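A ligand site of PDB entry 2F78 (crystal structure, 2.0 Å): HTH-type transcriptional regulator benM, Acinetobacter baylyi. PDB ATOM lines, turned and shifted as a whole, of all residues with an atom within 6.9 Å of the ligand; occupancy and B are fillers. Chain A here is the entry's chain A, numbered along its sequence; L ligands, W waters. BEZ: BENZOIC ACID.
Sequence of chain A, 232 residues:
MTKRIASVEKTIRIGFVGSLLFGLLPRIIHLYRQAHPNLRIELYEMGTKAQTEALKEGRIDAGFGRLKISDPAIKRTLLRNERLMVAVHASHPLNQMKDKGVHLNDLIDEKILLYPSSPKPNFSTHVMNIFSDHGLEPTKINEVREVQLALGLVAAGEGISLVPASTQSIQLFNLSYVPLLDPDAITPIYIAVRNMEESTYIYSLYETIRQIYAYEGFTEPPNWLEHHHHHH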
ATOM      1  N   PHE A  16      24.436  20.135 -15.672  1.00  0.00           N
ATOM      2  CA  PHE A  16      24.382  19.554 -14.321  1.00  0.00           C
ATOM      3  C   PHE A  16      24.146  18.045 -14.372  1.00  0.00           C
ATOM      4  O   PHE A  16      23.416  17.539 -15.233  1.00  0.00           O
ATOM      5  CB  PHE A  16      23.305  20.249 -13.476  1.00  0.00           C
ATOM      6  CG  PHE A  16      21.901  19.891 -13.885  1.00  0.00           C
ATOM      7  CD1 PHE A  16      21.237  18.841 -13.271  1.00  0.00           C
ATOM      8  CD2 PHE A  16      21.266  20.564 -14.911  1.00  0.00           C
ATOM      9  CE1 PHE A  16      19.971  18.478 -13.648  1.00  0.00           C
ATOM     10  CE2 PHE A  16      19.973  20.215 -15.298  1.00  0.00           C
ATOM     11  CZ  PHE A  16      19.339  19.182 -14.671  1.00  0.00           C
ATOM     12  N   VAL A  17      24.779  17.322 -13.447  1.00  0.00           N
ATOM     13  CA  VAL A  17      24.459  15.911 -13.212  1.00  0.00           C
ATOM     14  C   VAL A  17      23.129  15.796 -12.438  1.00  0.00           C
ATOM     15  O   VAL A  17      22.931  16.495 -11.443  1.00  0.00           O
ATOM     16  CB  VAL A  17      25.622  15.201 -12.438  1.00  0.00           C
ATOM     17  CG1 VAL A  17      25.157  13.921 -11.798  1.00  0.00           C
ATOM     18  CG2 VAL A  17      26.795  14.932 -13.376  1.00  0.00           C
ATOM     19  N   LEU A  20      22.220  16.009  -8.575  1.00  0.00           N
ATOM     20  CA  LEU A  20      22.367  17.297  -7.888  1.00  0.00           C
ATOM     21  C   LEU A  20      21.024  18.019  -7.678  1.00  0.00           C
ATOM     22  O   LEU A  20      20.925  18.952  -6.875  1.00  0.00           O
ATOM     23  CB  LEU A  20      23.363  18.203  -8.633  1.00  0.00           C
ATOM     24  CG  LEU A  20      24.765  17.634  -8.809  1.00  0.00           C
ATOM     25  CD1 LEU A  20      25.597  18.491  -9.738  1.00  0.00           C
ATOM     26  CD2 LEU A  20      25.468  17.485  -7.450  1.00  0.00           C
ATOM     27  N   LEU A  21      19.991  17.582  -8.391  1.00  0.00           N
ATOM     28  CA  LEU A  21      18.673  18.184  -8.202  1.00  0.00           C
ATOM     29  C   LEU A  21      18.116  17.892  -6.816  1.00  0.00           C
ATOM     30  O   LEU A  21      17.319  18.681  -6.320  1.00  0.00           O
ATOM     31  CB  LEU A  21      17.692  17.700  -9.274  1.00  0.00           C
ATOM     32  CG  LEU A  21      17.906  18.274 -10.683  1.00  0.00           C
ATOM     33  CD1 LEU A  21      16.968  17.593 -11.646  1.00  0.00           C
ATOM     34  CD2 LEU A  21      17.696  19.766 -10.705  1.00  0.00           C
ATOM     35  N   PHE A  22      18.546  16.792  -6.188  1.00  0.00           N
ATOM     36  CA  PHE A  22      18.080  16.446  -4.836  1.00  0.00           C
ATOM     37  C   PHE A  22      18.848  17.197  -3.740  1.00  0.00           C
ATOM     38  O   PHE A  22      18.506  17.091  -2.559  1.00  0.00           O
ATOM     39  CB  PHE A  22      18.167  14.939  -4.572  1.00  0.00           C
ATOM     40  CG  PHE A  22      17.372  14.115  -5.535  1.00  0.00           C
ATOM     41  CD1 PHE A  22      15.989  14.191  -5.570  1.00  0.00           C
ATOM     42  CD2 PHE A  22      18.018  13.237  -6.406  1.00  0.00           C
ATOM     43  CE1 PHE A  22      15.265  13.426  -6.469  1.00  0.00           C
ATOM     44  CE2 PHE A  22      17.307  12.471  -7.311  1.00  0.00           C
ATOM     45  CZ  PHE A  22      15.924  12.556  -7.345  1.00  0.00           C
ATOM     46  N   GLY A  23      19.878  17.933  -4.142  1.00  0.00           N
ATOM     47  CA  GLY A  23      20.642  18.784  -3.232  1.00  0.00           C
ATOM     48  C   GLY A  23      20.339  20.257  -3.387  1.00  0.00           C
ATOM     49  O   GLY A  23      19.174  20.666  -3.498  1.00  0.00           O
ATOM     50  N   LEU A  24      21.391  21.076  -3.443  1.00  0.00           N
ATOM     51  CA  LEU A  24      21.255  22.534  -3.386  1.00  0.00           C
ATOM     52  C   LEU A  24      21.090  23.202  -4.728  1.00  0.00           C
ATOM     53  O   LEU A  24      20.872  24.404  -4.764  1.00  0.00           O
ATOM     54  CB  LEU A  24      22.463  23.159  -2.679  1.00  0.00           C
ATOM     55  CG  LEU A  24      22.747  22.703  -1.244  1.00  0.00           C
ATOM     56  CD1 LEU A  24      24.042  23.303  -0.752  1.00  0.00           C
ATOM     57  CD2 LEU A  24      21.598  23.061  -0.312  1.00  0.00           C
ATOM     58  N   LEU A  25      21.189  22.451  -5.818  1.00  0.00           N
ATOM     59  CA  LEU A  25      21.129  23.049  -7.147  1.00  0.00           C
ATOM     60  C   LEU A  25      19.899  23.911  -7.398  1.00  0.00           C
ATOM     61  O   LEU A  25      20.035  25.065  -7.829  1.00  0.00           O
ATOM     62  CB  LEU A  25      21.252  21.976  -8.262  1.00  0.00           C
ATOM     63  CG  LEU A  25      21.291  22.527  -9.697  1.00  0.00           C
ATOM     64  CD1 LEU A  25      22.423  23.534  -9.879  1.00  0.00           C
ATOM     65  CD2 LEU A  25      21.411  21.383 -10.712  1.00  0.00           C
ATOM     66  N   PRO A  26      18.688  23.380  -7.167  1.00  0.00           N
ATOM     67  CA  PRO A  26      17.509  24.218  -7.423  1.00  0.00           C
ATOM     68  C   PRO A  26      17.435  25.532  -6.624  1.00  0.00           C
ATOM     69  O   PRO A  26      17.051  26.552  -7.198  1.00  0.00           O
ATOM     70  CB  PRO A  26      16.333  23.288  -7.069  1.00  0.00           C
ATOM     71  CG  PRO A  26      16.885  21.915  -7.294  1.00  0.00           C
ATOM     72  CD  PRO A  26      18.297  22.026  -6.751  1.00  0.00           C
ATOM     73  N   ILE A  28      19.960  27.239  -5.413  1.00  0.00           N
ATOM     74  CA  ILE A  28      21.040  28.055  -5.951  1.00  0.00           C
ATOM     75  C   ILE A  28      20.608  28.732  -7.265  1.00  0.00           C
ATOM     76  O   ILE A  28      20.797  29.927  -7.447  1.00  0.00           O
ATOM     77  CB  ILE A  28      22.325  27.217  -6.159  1.00  0.00           C
ATOM     78  CG1 ILE A  28      22.955  26.883  -4.809  1.00  0.00           C
ATOM     79  CG2 ILE A  28      23.334  27.972  -7.018  1.00  0.00           C
ATOM     80  CD1 ILE A  28      24.055  25.813  -4.880  1.00  0.00           C
ATOM     81  N   PHE A  64      28.167  21.659 -13.460  1.00  0.00           N
ATOM     82  CA  PHE A  64      28.211  21.071 -12.116  1.00  0.00           C
ATOM     83  C   PHE A  64      28.297  19.553 -12.228  1.00  0.00           C
ATOM     84  O   PHE A  64      27.321  18.905 -12.613  1.00  0.00           O
ATOM     85  CB  PHE A  64      26.964  21.461 -11.315  1.00  0.00           C
ATOM     86  CG  PHE A  64      26.882  22.914 -10.971  1.00  0.00           C
ATOM     87  CD1 PHE A  64      27.759  23.461 -10.030  1.00  0.00           C
ATOM     88  CD2 PHE A  64      25.929  23.738 -11.549  1.00  0.00           C
ATOM     89  CE1 PHE A  64      27.686  24.803  -9.690  1.00  0.00           C
ATOM     90  CE2 PHE A  64      25.843  25.081 -11.203  1.00  0.00           C
ATOM     91  CZ  PHE A  64      26.716  25.610 -10.287  1.00  0.00           C
ATOM     92  N   ARG A  66      30.502  15.569 -10.950  1.00  0.00           N
ATOM     93  CA  ARG A  66      30.944  14.720  -9.838  1.00  0.00           C
ATOM     94  C   ARG A  66      32.264  14.005 -10.099  1.00  0.00           C
ATOM     95  O   ARG A  66      32.735  13.251  -9.237  1.00  0.00           O
ATOM     96  CB  ARG A  66      29.890  13.650  -9.598  1.00  0.00           C
ATOM     97  CG  ARG A  66      28.520  14.187  -9.230  1.00  0.00           C
ATOM     98  CD  ARG A  66      28.387  14.263  -7.742  1.00  0.00           C
ATOM     99  NE  ARG A  66      27.015  14.077  -7.311  1.00  0.00           N
ATOM    100  CZ  ARG A  66      26.632  14.228  -6.051  1.00  0.00           C
ATOM    101  NH1 ARG A  66      27.510  14.542  -5.106  1.00  0.00           N
ATOM    102  NH2 ARG A  66      25.349  14.047  -5.746  1.00  0.00           N
ATOM    103  N   LEU A  79      33.613  22.117  -4.999  1.00  0.00           N
ATOM    104  CA  LEU A  79      32.699  22.900  -4.161  1.00  0.00           C
ATOM    105  C   LEU A  79      32.612  22.325  -2.747  1.00  0.00           C
ATOM    106  O   LEU A  79      32.849  23.020  -1.769  1.00  0.00           O
ATOM    107  CB  LEU A  79      31.299  22.958  -4.794  1.00  0.00           C
ATOM    108  CG  LEU A  79      31.221  23.728  -6.106  1.00  0.00           C
ATOM    109  CD1 LEU A  79      29.824  23.684  -6.724  1.00  0.00           C
ATOM    110  CD2 LEU A  79      31.671  25.153  -5.905  1.00  0.00           C
ATOM    111  N   ARG A  80      32.260  21.044  -2.675  1.00  0.00           N
ATOM    112  CA  ARG A  80      32.191  20.323  -1.415  1.00  0.00           C
ATOM    113  C   ARG A  80      32.196  18.814  -1.654  1.00  0.00           C
ATOM    114  O   ARG A  80      31.978  18.365  -2.777  1.00  0.00           O
ATOM    115  CB  ARG A  80      30.942  20.732  -0.603  1.00  0.00           C
ATOM    116  CG  ARG A  80      29.617  20.106  -1.023  1.00  0.00           C
ATOM    117  CD  ARG A  80      28.492  20.706  -0.193  1.00  0.00           C
ATOM    118  NE  ARG A  80      27.169  20.349  -0.677  1.00  0.00           N
ATOM    119  CZ  ARG A  80      26.398  19.371  -0.184  1.00  0.00           C
ATOM    120  NH1 ARG A  80      26.798  18.635   0.845  1.00  0.00           N
ATOM    121  NH2 ARG A  80      25.218  19.140  -0.723  1.00  0.00           N
ATOM    122  N   GLU A  82      30.170  15.630  -0.513  1.00  0.00           N
ATOM    123  CA  GLU A  82      28.917  15.187   0.062  1.00  0.00           C
ATOM    124  C   GLU A  82      29.145  13.832   0.691  1.00  0.00           C
ATOM    125  O   GLU A  82      29.819  12.972   0.099  1.00  0.00           O
ATOM    126  CB  GLU A  82      27.879  15.105  -1.045  1.00  0.00           C
ATOM    127  CG  GLU A  82      26.488  15.000  -0.507  1.00  0.00           C
ATOM    128  CD  GLU A  82      25.432  15.066  -1.577  1.00  0.00           C
ATOM    129  OE1 GLU A  82      25.786  15.113  -2.780  1.00  0.00           O
ATOM    130  OE2 GLU A  82      24.255  15.072  -1.207  1.00  0.00           O
ATOM    131  N   SER A 166      22.096  13.678   0.090  1.00  0.00           N
ATOM    132  CA  SER A 166      20.950  14.476  -0.381  1.00  0.00           C
ATOM    133  C   SER A 166      19.826  13.634  -1.008  1.00  0.00           C
ATOM    134  O   SER A 166      18.759  14.156  -1.320  1.00  0.00           O
ATOM    135  CB  SER A 166      21.413  15.522  -1.382  1.00  0.00           C
ATOM    136  OG  SER A 166      22.106  14.901  -2.441  1.00  0.00           O
ATOM    137  N   ILE A 189      31.356  17.386  -5.475  1.00  0.00           N
ATOM    138  CA  ILE A 189      30.615  18.228  -6.390  1.00  0.00           C
ATOM    139  C   ILE A 189      31.635  19.249  -6.904  1.00  0.00           C
ATOM    140  O   ILE A 189      32.316  19.877  -6.106  1.00  0.00           O
ATOM    141  CB  ILE A 189      29.390  18.921  -5.698  1.00  0.00           C
ATOM    142  CG1 ILE A 189      28.558  17.896  -4.910  1.00  0.00           C
ATOM    143  CG2 ILE A 189      28.488  19.615  -6.717  1.00  0.00           C
ATOM    144  CD1 ILE A 189      27.462  18.502  -4.069  1.00  0.00           C
ATOM    145  N   TYR A 190      31.767  19.346  -8.218  1.00  0.00           N
ATOM    146  CA  TYR A 190      32.682  20.315  -8.840  1.00  0.00           C
ATOM    147  C   TYR A 190      31.890  21.312  -9.655  1.00  0.00           C
ATOM    148  O   TYR A 190      30.822  20.990 -10.179  1.00  0.00           O
ATOM    149  CB  TYR A 190      33.660  19.620  -9.796  1.00  0.00           C
ATOM    150  CG  TYR A 190      34.591  18.620  -9.154  1.00  0.00           C
ATOM    151  CD1 TYR A 190      35.809  19.010  -8.610  1.00  0.00           C
ATOM    152  CD2 TYR A 190      34.257  17.272  -9.123  1.00  0.00           C
ATOM    153  CE1 TYR A 190      36.676  18.092  -8.029  1.00  0.00           C
ATOM    154  CE2 TYR A 190      35.118  16.334  -8.535  1.00  0.00           C
ATOM    155  CZ  TYR A 190      36.317  16.754  -7.985  1.00  0.00           C
ATOM    156  OH  TYR A 190      37.163  15.819  -7.413  1.00  0.00           O
ATOM    157  N   ILE A 191      32.425  22.523  -9.780  1.00  0.00           N
ATOM    158  CA  ILE A 191      31.957  23.428 -10.834  1.00  0.00           C
ATOM    159  C   ILE A 191      33.096  23.572 -11.838  1.00  0.00           C
ATOM    160  O   ILE A 191      34.222  23.877 -11.476  1.00  0.00           O
ATOM    161  CB  ILE A 191      31.469  24.805 -10.316  1.00  0.00           C
ATOM    162  CG1 ILE A 191      31.010  25.662 -11.497  1.00  0.00           C
ATOM    163  CG2 ILE A 191      32.540  25.550  -9.491  1.00  0.00           C
ATOM    164  CD1 ILE A 191      30.088  26.775 -11.110  1.00  0.00           C
ATOM    165  N   ILE A 209      26.497  30.623  -4.820  1.00  0.00           N
ATOM    166  CA  ILE A 209      26.936  29.370  -4.179  1.00  0.00           C
ATOM    167  C   ILE A 209      27.574  29.660  -2.823  1.00  0.00           C
ATOM    168  O   ILE A 209      27.249  28.998  -1.837  1.00  0.00           O
ATOM    169  CB  ILE A 209      27.935  28.606  -5.069  1.00  0.00           C
ATOM    170  CG1 ILE A 209      27.286  28.203  -6.405  1.00  0.00           C
ATOM    171  CG2 ILE A 209      28.483  27.355  -4.343  1.00  0.00           C
ATOM    172  CD1 ILE A 209      28.296  27.750  -7.482  1.00  0.00           C
ATOM    173  N   TYR A 213      26.137  28.338   0.694  1.00  0.00           N
ATOM    174  CA  TYR A 213      27.094  27.553   1.480  1.00  0.00           C
ATOM    175  C   TYR A 213      27.312  28.145   2.882  1.00  0.00           C
ATOM    176  O   TYR A 213      27.444  27.407   3.853  1.00  0.00           O
ATOM    177  CB  TYR A 213      28.420  27.395   0.716  1.00  0.00           C
ATOM    178  CG  TYR A 213      28.440  26.223  -0.242  1.00  0.00           C
ATOM    179  CD1 TYR A 213      27.280  25.810  -0.894  1.00  0.00           C
ATOM    180  CD2 TYR A 213      29.622  25.529  -0.500  1.00  0.00           C
ATOM    181  CE1 TYR A 213      27.291  24.740  -1.763  1.00  0.00           C
ATOM    182  CE2 TYR A 213      29.636  24.460  -1.378  1.00  0.00           C
ATOM    183  CZ  TYR A 213      28.458  24.066  -2.003  1.00  0.00           C
ATOM    184  OH  TYR A 213      28.441  23.009  -2.881  1.00  0.00           O
ATOM    185  N   PHE A 218      28.915  25.719   5.827  1.00  0.00           N
ATOM    186  CA  PHE A 218      30.075  25.107   5.192  1.00  0.00           C
ATOM    187  C   PHE A 218      31.240  26.099   5.321  1.00  0.00           C
ATOM    188  O   PHE A 218      31.059  27.297   5.095  1.00  0.00           O
ATOM    189  CB  PHE A 218      29.798  24.760   3.711  1.00  0.00           C
ATOM    190  CG  PHE A 218      28.686  23.724   3.481  1.00  0.00           C
ATOM    191  CD1 PHE A 218      28.473  22.662   4.350  1.00  0.00           C
ATOM    192  CD2 PHE A 218      27.868  23.808   2.352  1.00  0.00           C
ATOM    193  CE1 PHE A 218      27.458  21.719   4.121  1.00  0.00           C
ATOM    194  CE2 PHE A 218      26.849  22.886   2.113  1.00  0.00           C
ATOM    195  CZ  PHE A 218      26.640  21.841   3.006  1.00  0.00           C
HETATM  196  C   BEZ L   1      25.301  21.174  -3.831  1.00  0.00           C
HETATM  197  O1  BEZ L   1      26.249  21.626  -2.913  1.00  0.00           O
HETATM  198  O2  BEZ L   1      24.431  20.250  -3.490  1.00  0.00           O
HETATM  199  C1  BEZ L   1      25.318  21.759  -5.196  1.00  0.00           C
HETATM  200  C2  BEZ L   1      25.979  22.968  -5.403  1.00  0.00           C
HETATM  201  C3  BEZ L   1      26.008  23.512  -6.670  1.00  0.00           C
HETATM  202  C4  BEZ L   1      25.371  22.876  -7.708  1.00  0.00           C
HETATM  203  C5  BEZ L   1      24.714  21.668  -7.511  1.00  0.00           C
HETATM  204  C6  BEZ L   1      24.683  21.104  -6.246  1.00  0.00           C
HETATM  205  O   HOH W   1      23.757  17.427  -4.233  1.00  0.00           O
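Residues that only touch the ligand: Phe 64 (3.4 Å), Ile 189 (3.4 Å), Ile 28 (3.5 Å), Leu 25 (3.6 Å), Leu 79 (3.8 Å) and Leu 20 (3.9 Å).
Hydrophobic or aromatic side chains within 4 Å of the ligand: Leu 20, Leu 24, Leu 25, Ile 28, Phe 64, Leu 79, Ile 189 and Tyr 213.
Of the 22 residues printed, 9 come within 4 Å of the ligand.
The nearest printed residue that does not touch the ligand is Gly 23 (4.1 Å).
O of Phe 64 lies within hydrogen-bond range of N of Val 17, 3.1 Å away.
The backbone carbonyl oxygen of Ile 189 lies within hydrogen-bond range of the backbone NH of Leu 79, at 2.8 Å.
O of Arg 80 is in hydrogen-bond range of N of Ile 189, at 2.9 Å.
The backbone carbonyl oxygen of Tyr 213 sits at hydrogen-bond distance from the backbone NH of Phe 218, 3.0 Å away.
Water W1 bridges O2 of the ligand and OE1 of Glu 82.
The guanidinium group of Arg 80 lies within salt-bridge range of an oxygen (O1) of the ligand (2.7 Å).
The side-chain hydroxyl (OH) of Tyr 213 sits at hydrogen-bond distance from an oxygen (O1) of the ligand (2.6 Å).
The backbone NH (N) of Leu 24 is in hydrogen-bond range of an oxygen (O2) of the ligand, 3.2 Å away.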
